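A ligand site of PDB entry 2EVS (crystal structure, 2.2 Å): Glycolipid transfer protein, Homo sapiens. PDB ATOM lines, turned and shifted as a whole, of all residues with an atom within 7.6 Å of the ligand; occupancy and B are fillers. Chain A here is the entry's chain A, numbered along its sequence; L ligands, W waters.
NZ of Lys 55 is in hydrogen-bond range of O3 of the ligand (3.0 Å).
OH of Tyr 207 sits at hydrogen-bond distance from O6 of the ligand (2.5 Å).
OD1 of Asp 48 is in hydrogen-bond range of O2 of the ligand (2.8 Å).
The side-chain amide oxygen (OD1) of Asn 52 sits at hydrogen-bond distance from an oxygen (O3) of the ligand (2.4 Å).
The backbone carbonyl oxygen (O) of Tyr 139 lies within hydrogen-bond range of the backbone NH (N) of Val 209, 2.9 Å away.
The indole nitrogen of Trp 96 is in hydrogen-bond range of the side-chain hydroxyl of Tyr 207, at 2.9 Å.
Residues that only touch the ligand: Leu 92 (3.8 Å), Trp 96 (3.7 Å) and Val 209 (3.6 Å).
Seven residues have an atom within 4 Å of the ligand: Asp 48, Asn 52, Lys 55, Leu 92, Trp 96, Tyr 207 and Val 209.
The nearest printed residue that does not touch the ligand is Ala 93 (4.7 Å).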
ATOM      1  N   ALA A  47       8.971  16.915  28.955  1.00  0.00           N
ATOM      2  CA  ALA A  47      10.362  17.302  29.001  1.00  0.00           C
ATOM      3  C   ALA A  47      10.897  17.729  27.645  1.00  0.00           C
ATOM      4  O   ALA A  47      11.707  18.626  27.578  1.00  0.00           O
ATOM      5  CB  ALA A  47      11.198  16.146  29.551  1.00  0.00           C
ATOM      6  N   ASP A  48      10.440  17.120  26.579  1.00  0.00           N
ATOM      7  CA  ASP A  48      10.849  17.512  25.239  1.00  0.00           C
ATOM      8  C   ASP A  48      10.386  18.906  24.861  1.00  0.00           C
ATOM      9  O   ASP A  48      11.187  19.719  24.385  1.00  0.00           O
ATOM     10  CB  ASP A  48      10.306  16.554  24.182  1.00  0.00           C
ATOM     11  CG  ASP A  48      11.075  16.616  22.895  1.00  0.00           C
ATOM     12  OD1 ASP A  48      12.350  16.596  22.948  1.00  0.00           O
ATOM     13  OD2 ASP A  48      10.440  16.666  21.845  1.00  0.00           O
ATOM     14  N   ILE A  49       9.062  19.147  25.002  1.00  0.00           N
ATOM     15  CA  ILE A  49       8.460  20.466  24.815  1.00  0.00           C
ATOM     16  C   ILE A  49       9.186  21.513  25.651  1.00  0.00           C
ATOM     17  O   ILE A  49       9.574  22.573  25.175  1.00  0.00           O
ATOM     18  CB  ILE A  49       6.916  20.455  25.129  1.00  0.00           C
ATOM     19  CG1 ILE A  49       6.136  19.804  23.984  1.00  0.00           C
ATOM     20  CG2 ILE A  49       6.350  21.874  25.346  1.00  0.00           C
ATOM     21  CD1 ILE A  49       4.868  19.138  24.395  1.00  0.00           C
ATOM     22  N   GLY A  51      12.250  21.491  27.131  1.00  0.00           N
ATOM     23  CA  GLY A  51      13.617  21.702  26.748  1.00  0.00           C
ATOM     24  C   GLY A  51      13.697  22.592  25.520  1.00  0.00           C
ATOM     25  O   GLY A  51      14.594  23.405  25.428  1.00  0.00           O
ATOM     26  N   ASN A  52      12.783  22.396  24.566  1.00  0.00           N
ATOM     27  CA  ASN A  52      12.805  23.214  23.331  1.00  0.00           C
ATOM     28  C   ASN A  52      12.407  24.658  23.623  1.00  0.00           C
ATOM     29  O   ASN A  52      13.009  25.585  23.124  1.00  0.00           O
ATOM     30  CB  ASN A  52      11.979  22.603  22.204  1.00  0.00           C
ATOM     31  CG  ASN A  52      12.716  21.490  21.512  1.00  0.00           C
ATOM     32  OD1 ASN A  52      13.955  21.552  21.388  1.00  0.00           O
ATOM     33  ND2 ASN A  52      11.965  20.446  21.038  1.00  0.00           N
ATOM     34  N   ILE A  53      11.432  24.839  24.511  1.00  0.00           N
ATOM     35  CA  ILE A  53      11.056  26.202  24.962  1.00  0.00           C
ATOM     36  C   ILE A  53      12.272  26.915  25.586  1.00  0.00           C
ATOM     37  O   ILE A  53      12.575  28.049  25.229  1.00  0.00           O
ATOM     38  CB  ILE A  53       9.869  26.175  25.966  1.00  0.00           C
ATOM     39  CG1 ILE A  53       8.576  25.749  25.240  1.00  0.00           C
ATOM     40  CG2 ILE A  53       9.719  27.537  26.672  1.00  0.00           C
ATOM     41  CD1 ILE A  53       7.430  25.364  26.156  1.00  0.00           C
ATOM     42  N   LYS A  55      15.565  26.329  25.172  1.00  0.00           N
ATOM     43  CA  LYS A  55      16.583  26.628  24.161  1.00  0.00           C
ATOM     44  C   LYS A  55      16.242  27.860  23.317  1.00  0.00           C
ATOM     45  O   LYS A  55      17.136  28.587  22.888  1.00  0.00           O
ATOM     46  CB  LYS A  55      16.792  25.496  23.195  1.00  0.00           C
ATOM     47  CG  LYS A  55      17.432  24.275  23.743  1.00  0.00           C
ATOM     48  CD  LYS A  55      17.540  23.266  22.593  1.00  0.00           C
ATOM     49  CE  LYS A  55      18.044  21.930  22.980  1.00  0.00           C
ATOM     50  NZ  LYS A  55      18.015  21.070  21.743  1.00  0.00           N
ATOM     51  N   LYS A  87      19.553  23.526  10.676  1.00  0.00           N
ATOM     52  CA  LYS A  87      19.829  22.585  11.761  1.00  0.00           C
ATOM     53  C   LYS A  87      20.697  23.228  12.820  1.00  0.00           C
ATOM     54  O   LYS A  87      21.787  22.749  13.130  1.00  0.00           O
ATOM     55  CB  LYS A  87      20.489  21.296  11.248  1.00  0.00           C
ATOM     56  CG  LYS A  87      20.190  20.089  12.116  1.00  0.00           C
ATOM     57  CD  LYS A  87      20.805  18.812  11.554  1.00  0.00           C
ATOM     58  CE  LYS A  87      20.638  17.663  12.554  1.00  0.00           C
ATOM     59  NZ  LYS A  87      21.103  16.316  12.051  1.00  0.00           N
ATOM     60  N   GLY A  89      20.561  25.727  16.672  1.00  0.00           N
ATOM     61  CA  GLY A  89      20.085  26.621  17.701  1.00  0.00           C
ATOM     62  C   GLY A  89      18.587  26.680  17.869  1.00  0.00           C
ATOM     63  O   GLY A  89      17.919  25.655  17.879  1.00  0.00           O
ATOM     64  N   LEU A  92      16.186  25.234  15.188  1.00  0.00           N
ATOM     65  CA  LEU A  92      15.966  23.787  15.275  1.00  0.00           C
ATOM     66  C   LEU A  92      15.041  23.412  16.438  1.00  0.00           C
ATOM     67  O   LEU A  92      14.167  22.547  16.297  1.00  0.00           O
ATOM     68  CB  LEU A  92      17.308  23.064  15.429  1.00  0.00           C
ATOM     69  CG  LEU A  92      17.306  21.524  15.455  1.00  0.00           C
ATOM     70  CD1 LEU A  92      16.691  20.983  14.222  1.00  0.00           C
ATOM     71  CD2 LEU A  92      18.763  20.996  15.620  1.00  0.00           C
ATOM     72  N   ALA A  93      15.272  24.044  17.597  1.00  0.00           N
ATOM     73  CA  ALA A  93      14.396  23.898  18.742  1.00  0.00           C
ATOM     74  C   ALA A  93      12.916  24.244  18.387  1.00  0.00           C
ATOM     75  O   ALA A  93      12.008  23.449  18.683  1.00  0.00           O
ATOM     76  CB  ALA A  93      14.903  24.713  19.911  1.00  0.00           C
ATOM     77  N   LEU A  94      12.703  25.351  17.709  1.00  0.00           N
ATOM     78  CA  LEU A  94      11.344  25.727  17.264  1.00  0.00           C
ATOM     79  C   LEU A  94      10.792  24.740  16.236  1.00  0.00           C
ATOM     80  O   LEU A  94       9.596  24.453  16.229  1.00  0.00           O
ATOM     81  CB  LEU A  94      11.286  27.175  16.779  1.00  0.00           C
ATOM     82  CG  LEU A  94       9.930  27.742  16.311  1.00  0.00           C
ATOM     83  CD1 LEU A  94       8.857  27.667  17.445  1.00  0.00           C
ATOM     84  CD2 LEU A  94      10.049  29.174  15.756  1.00  0.00           C
ATOM     85  N   MET A  95      11.672  24.200  15.399  1.00  0.00           N
ATOM     86  CA  MET A  95      11.277  23.187  14.389  1.00  0.00           C
ATOM     87  C   MET A  95      10.650  21.982  15.059  1.00  0.00           C
ATOM     88  O   MET A  95       9.655  21.404  14.577  1.00  0.00           O
ATOM     89  CB  MET A  95      12.476  22.741  13.526  1.00  0.00           C
ATOM     90  CG  MET A  95      12.127  21.999  12.244  1.00  0.00           C
ATOM     91  SD  MET A  95      13.532  21.215  11.493  1.00  0.00           S
ATOM     92  CE  MET A  95      13.663  19.811  12.583  1.00  0.00           C
ATOM     93  N   TRP A  96      11.272  21.558  16.148  1.00  0.00           N
ATOM     94  CA  TRP A  96      10.743  20.476  16.959  1.00  0.00           C
ATOM     95  C   TRP A  96       9.587  20.928  17.832  1.00  0.00           C
ATOM     96  O   TRP A  96       8.575  20.225  17.941  1.00  0.00           O
ATOM     97  CB  TRP A  96      11.863  19.839  17.758  1.00  0.00           C
ATOM     98  CG  TRP A  96      12.725  18.972  16.884  1.00  0.00           C
ATOM     99  CD1 TRP A  96      13.872  19.309  16.254  1.00  0.00           C
ATOM    100  CD2 TRP A  96      12.437  17.624  16.483  1.00  0.00           C
ATOM    101  NE1 TRP A  96      14.343  18.261  15.515  1.00  0.00           N
ATOM    102  CE2 TRP A  96      13.484  17.211  15.633  1.00  0.00           C
ATOM    103  CE3 TRP A  96      11.409  16.714  16.782  1.00  0.00           C
ATOM    104  CZ2 TRP A  96      13.544  15.920  15.108  1.00  0.00           C
ATOM    105  CZ3 TRP A  96      11.444  15.463  16.239  1.00  0.00           C
ATOM    106  CH2 TRP A  96      12.512  15.070  15.408  1.00  0.00           C
ATOM    107  N   LEU A  97       9.689  22.130  18.426  1.00  0.00           N
ATOM    108  CA  LEU A  97       8.627  22.604  19.321  1.00  0.00           C
ATOM    109  C   LEU A  97       7.258  22.636  18.625  1.00  0.00           C
ATOM    110  O   LEU A  97       6.289  22.214  19.217  1.00  0.00           O
ATOM    111  CB  LEU A  97       8.951  23.949  19.922  1.00  0.00           C
ATOM    112  CG  LEU A  97       7.894  24.572  20.850  1.00  0.00           C
ATOM    113  CD1 LEU A  97       7.647  23.716  22.073  1.00  0.00           C
ATOM    114  CD2 LEU A  97       8.314  25.986  21.301  1.00  0.00           C
ATOM    115  N   ARG A  99       5.925  20.803  16.390  1.00  0.00           N
ATOM    116  CA  ARG A  99       5.363  19.470  16.281  1.00  0.00           C
ATOM    117  C   ARG A  99       4.730  19.022  17.597  1.00  0.00           C
ATOM    118  O   ARG A  99       3.686  18.347  17.593  1.00  0.00           O
ATOM    119  CB  ARG A  99       6.442  18.457  15.902  1.00  0.00           C
ATOM    120  CG  ARG A  99       7.115  18.785  14.599  1.00  0.00           C
ATOM    121  CD  ARG A  99       8.369  17.955  14.392  1.00  0.00           C
ATOM    122  NE  ARG A  99       8.900  18.259  13.080  1.00  0.00           N
ATOM    123  CZ  ARG A  99      10.114  17.944  12.652  1.00  0.00           C
ATOM    124  NH1 ARG A  99      10.935  17.232  13.402  1.00  0.00           N
ATOM    125  NH2 ARG A  99      10.451  18.240  11.410  1.00  0.00           N
ATOM    126  N   LEU A 136       4.033  13.751  15.149  1.00  0.00           N
ATOM    127  CA  LEU A 136       5.400  13.447  15.603  1.00  0.00           C
ATOM    128  C   LEU A 136       6.035  12.175  15.089  1.00  0.00           C
ATOM    129  O   LEU A 136       7.227  12.122  14.876  1.00  0.00           O
ATOM    130  CB  LEU A 136       5.406  13.385  17.118  1.00  0.00           C
ATOM    131  CG  LEU A 136       5.322  14.678  17.911  1.00  0.00           C
ATOM    132  CD1 LEU A 136       4.862  14.363  19.338  1.00  0.00           C
ATOM    133  CD2 LEU A 136       6.707  15.416  17.909  1.00  0.00           C
ATOM    134  N   TYR A 139       8.814  11.521  12.445  1.00  0.00           N
ATOM    135  CA  TYR A 139      10.111  12.109  12.788  1.00  0.00           C
ATOM    136  C   TYR A 139      10.865  11.353  13.894  1.00  0.00           C
ATOM    137  O   TYR A 139      11.931  11.798  14.326  1.00  0.00           O
ATOM    138  CB  TYR A 139       9.836  13.575  13.229  1.00  0.00           C
ATOM    139  CG  TYR A 139       9.109  14.365  12.185  1.00  0.00           C
ATOM    140  CD1 TYR A 139       9.744  14.754  11.005  1.00  0.00           C
ATOM    141  CD2 TYR A 139       7.789  14.670  12.315  1.00  0.00           C
ATOM    142  CE1 TYR A 139       9.076  15.463  10.048  1.00  0.00           C
ATOM    143  CE2 TYR A 139       7.107  15.397  11.363  1.00  0.00           C
ATOM    144  CZ  TYR A 139       7.760  15.775  10.251  1.00  0.00           C
ATOM    145  OH  TYR A 139       7.069  16.483   9.330  1.00  0.00           O
ATOM    146  N   HIS A 140      10.318  10.228  14.347  1.00  0.00           N
ATOM    147  CA  HIS A 140      10.909   9.444  15.449  1.00  0.00           C
ATOM    148  C   HIS A 140      11.335   8.072  14.931  1.00  0.00           C
ATOM    149  O   HIS A 140      10.540   7.378  14.284  1.00  0.00           O
ATOM    150  CB  HIS A 140       9.879   9.230  16.539  1.00  0.00           C
ATOM    151  CG  HIS A 140       9.614  10.440  17.376  1.00  0.00           C
ATOM    152  ND1 HIS A 140       8.582  10.513  18.282  1.00  0.00           N
ATOM    153  CD2 HIS A 140      10.263  11.631  17.450  1.00  0.00           C
ATOM    154  CE1 HIS A 140       8.619  11.691  18.889  1.00  0.00           C
ATOM    155  NE2 HIS A 140       9.609  12.387  18.388  1.00  0.00           N
ATOM    156  N   VAL A 144      12.617   5.869  19.944  1.00  0.00           N
ATOM    157  CA  VAL A 144      11.833   6.969  20.459  1.00  0.00           C
ATOM    158  C   VAL A 144      10.319   6.662  20.322  1.00  0.00           C
ATOM    159  O   VAL A 144       9.519   6.989  21.209  1.00  0.00           O
ATOM    160  CB  VAL A 144      12.197   8.297  19.772  1.00  0.00           C
ATOM    161  CG1 VAL A 144      11.274   9.394  20.228  1.00  0.00           C
ATOM    162  CG2 VAL A 144      13.595   8.674  20.117  1.00  0.00           C
ATOM    163  N   PHE A 148       7.484   6.798  23.368  1.00  0.00           N
ATOM    164  CA  PHE A 148       6.274   7.631  23.303  1.00  0.00           C
ATOM    165  C   PHE A 148       5.042   6.783  23.320  1.00  0.00           C
ATOM    166  O   PHE A 148       4.021   7.184  23.899  1.00  0.00           O
ATOM    167  CB  PHE A 148       6.267   8.519  22.056  1.00  0.00           C
ATOM    168  CG  PHE A 148       7.005   9.821  22.219  1.00  0.00           C
ATOM    169  CD1 PHE A 148       8.374   9.842  22.358  1.00  0.00           C
ATOM    170  CD2 PHE A 148       6.310  11.034  22.216  1.00  0.00           C
ATOM    171  CE1 PHE A 148       9.041  11.022  22.499  1.00  0.00           C
ATOM    172  CE2 PHE A 148       6.990  12.239  22.347  1.00  0.00           C
ATOM    173  CZ  PHE A 148       8.358  12.228  22.492  1.00  0.00           C
ATOM    174  N   TYR A 207      14.543  14.731   9.025  1.00  0.00           N
ATOM    175  CA  TYR A 207      15.248  13.621   9.648  1.00  0.00           C
ATOM    176  C   TYR A 207      14.520  13.108  10.894  1.00  0.00           C
ATOM    177  O   TYR A 207      13.728  13.807  11.535  1.00  0.00           O
ATOM    178  CB  TYR A 207      16.707  13.984  10.017  1.00  0.00           C
ATOM    179  CG  TYR A 207      16.805  14.907  11.205  1.00  0.00           C
ATOM    180  CD1 TYR A 207      17.131  14.436  12.468  1.00  0.00           C
ATOM    181  CD2 TYR A 207      16.565  16.276  11.047  1.00  0.00           C
ATOM    182  CE1 TYR A 207      17.199  15.319  13.573  1.00  0.00           C
ATOM    183  CE2 TYR A 207      16.629  17.144  12.120  1.00  0.00           C
ATOM    184  CZ  TYR A 207      16.907  16.678  13.364  1.00  0.00           C
ATOM    185  OH  TYR A 207      16.986  17.613  14.381  1.00  0.00           O
ATOM    186  N   LYS A 208      14.845  11.872  11.240  1.00  0.00           N
ATOM    187  CA  LYS A 208      14.255  11.182  12.360  1.00  0.00           C
ATOM    188  C   LYS A 208      15.268  11.135  13.469  1.00  0.00           C
ATOM    189  O   LYS A 208      16.483  11.000  13.227  1.00  0.00           O
ATOM    190  CB  LYS A 208      13.941   9.749  11.993  1.00  0.00           C
ATOM    191  CG  LYS A 208      12.783   9.536  11.057  1.00  0.00           C
ATOM    192  CD  LYS A 208      12.768   8.093  10.653  1.00  0.00           C
ATOM    193  CE  LYS A 208      11.449   7.644  10.119  1.00  0.00           C
ATOM    194  NZ  LYS A 208      11.082   8.405   8.872  1.00  0.00           N
ATOM    195  N   VAL A 209      14.768  11.251  14.684  1.00  0.00           N
ATOM    196  CA  VAL A 209      15.548  10.903  15.848  1.00  0.00           C
ATOM    197  C   VAL A 209      14.824   9.744  16.509  1.00  0.00           C
ATOM    198  O   VAL A 209      15.468   8.789  16.827  1.00  0.00           O
ATOM    199  CB  VAL A 209      15.715  12.066  16.837  1.00  0.00           C
ATOM    200  CG1 VAL A 209      16.192  13.293  16.083  1.00  0.00           C
ATOM    201  CG2 VAL A 209      14.438  12.349  17.516  1.00  0.00           C
HETATM  202  C1  LIG L   1      14.951  16.165  19.873  1.00  0.00           C
HETATM  203  C2  LIG L   1      14.594  17.543  20.468  1.00  0.00           C
HETATM  204  C3  LIG L   1      15.327  18.712  19.816  1.00  0.00           C
HETATM  205  C4  LIG L   1      16.719  18.271  19.353  1.00  0.00           C
HETATM  206  C5  LIG L   1      16.568  17.206  18.303  1.00  0.00           C
HETATM  207  C6  LIG L   1      17.900  16.618  17.843  1.00  0.00           C
HETATM  208  O1  LIG L   1      13.815  15.369  19.571  1.00  0.00           O
HETATM  209  O2  LIG L   1      13.194  17.773  20.544  1.00  0.00           O
HETATM  210  O3  LIG L   1      15.471  19.797  20.715  1.00  0.00           O
HETATM  211  O4  LIG L   1      17.336  19.373  18.721  1.00  0.00           O
HETATM  212  O5  LIG L   1      15.694  16.152  18.675  1.00  0.00           O
HETATM  213  O6  LIG L   1      17.851  16.473  16.442  1.00  0.00           O
HETATM  214  O   HOH W   1      19.901  19.531  19.043  1.00  0.00           O
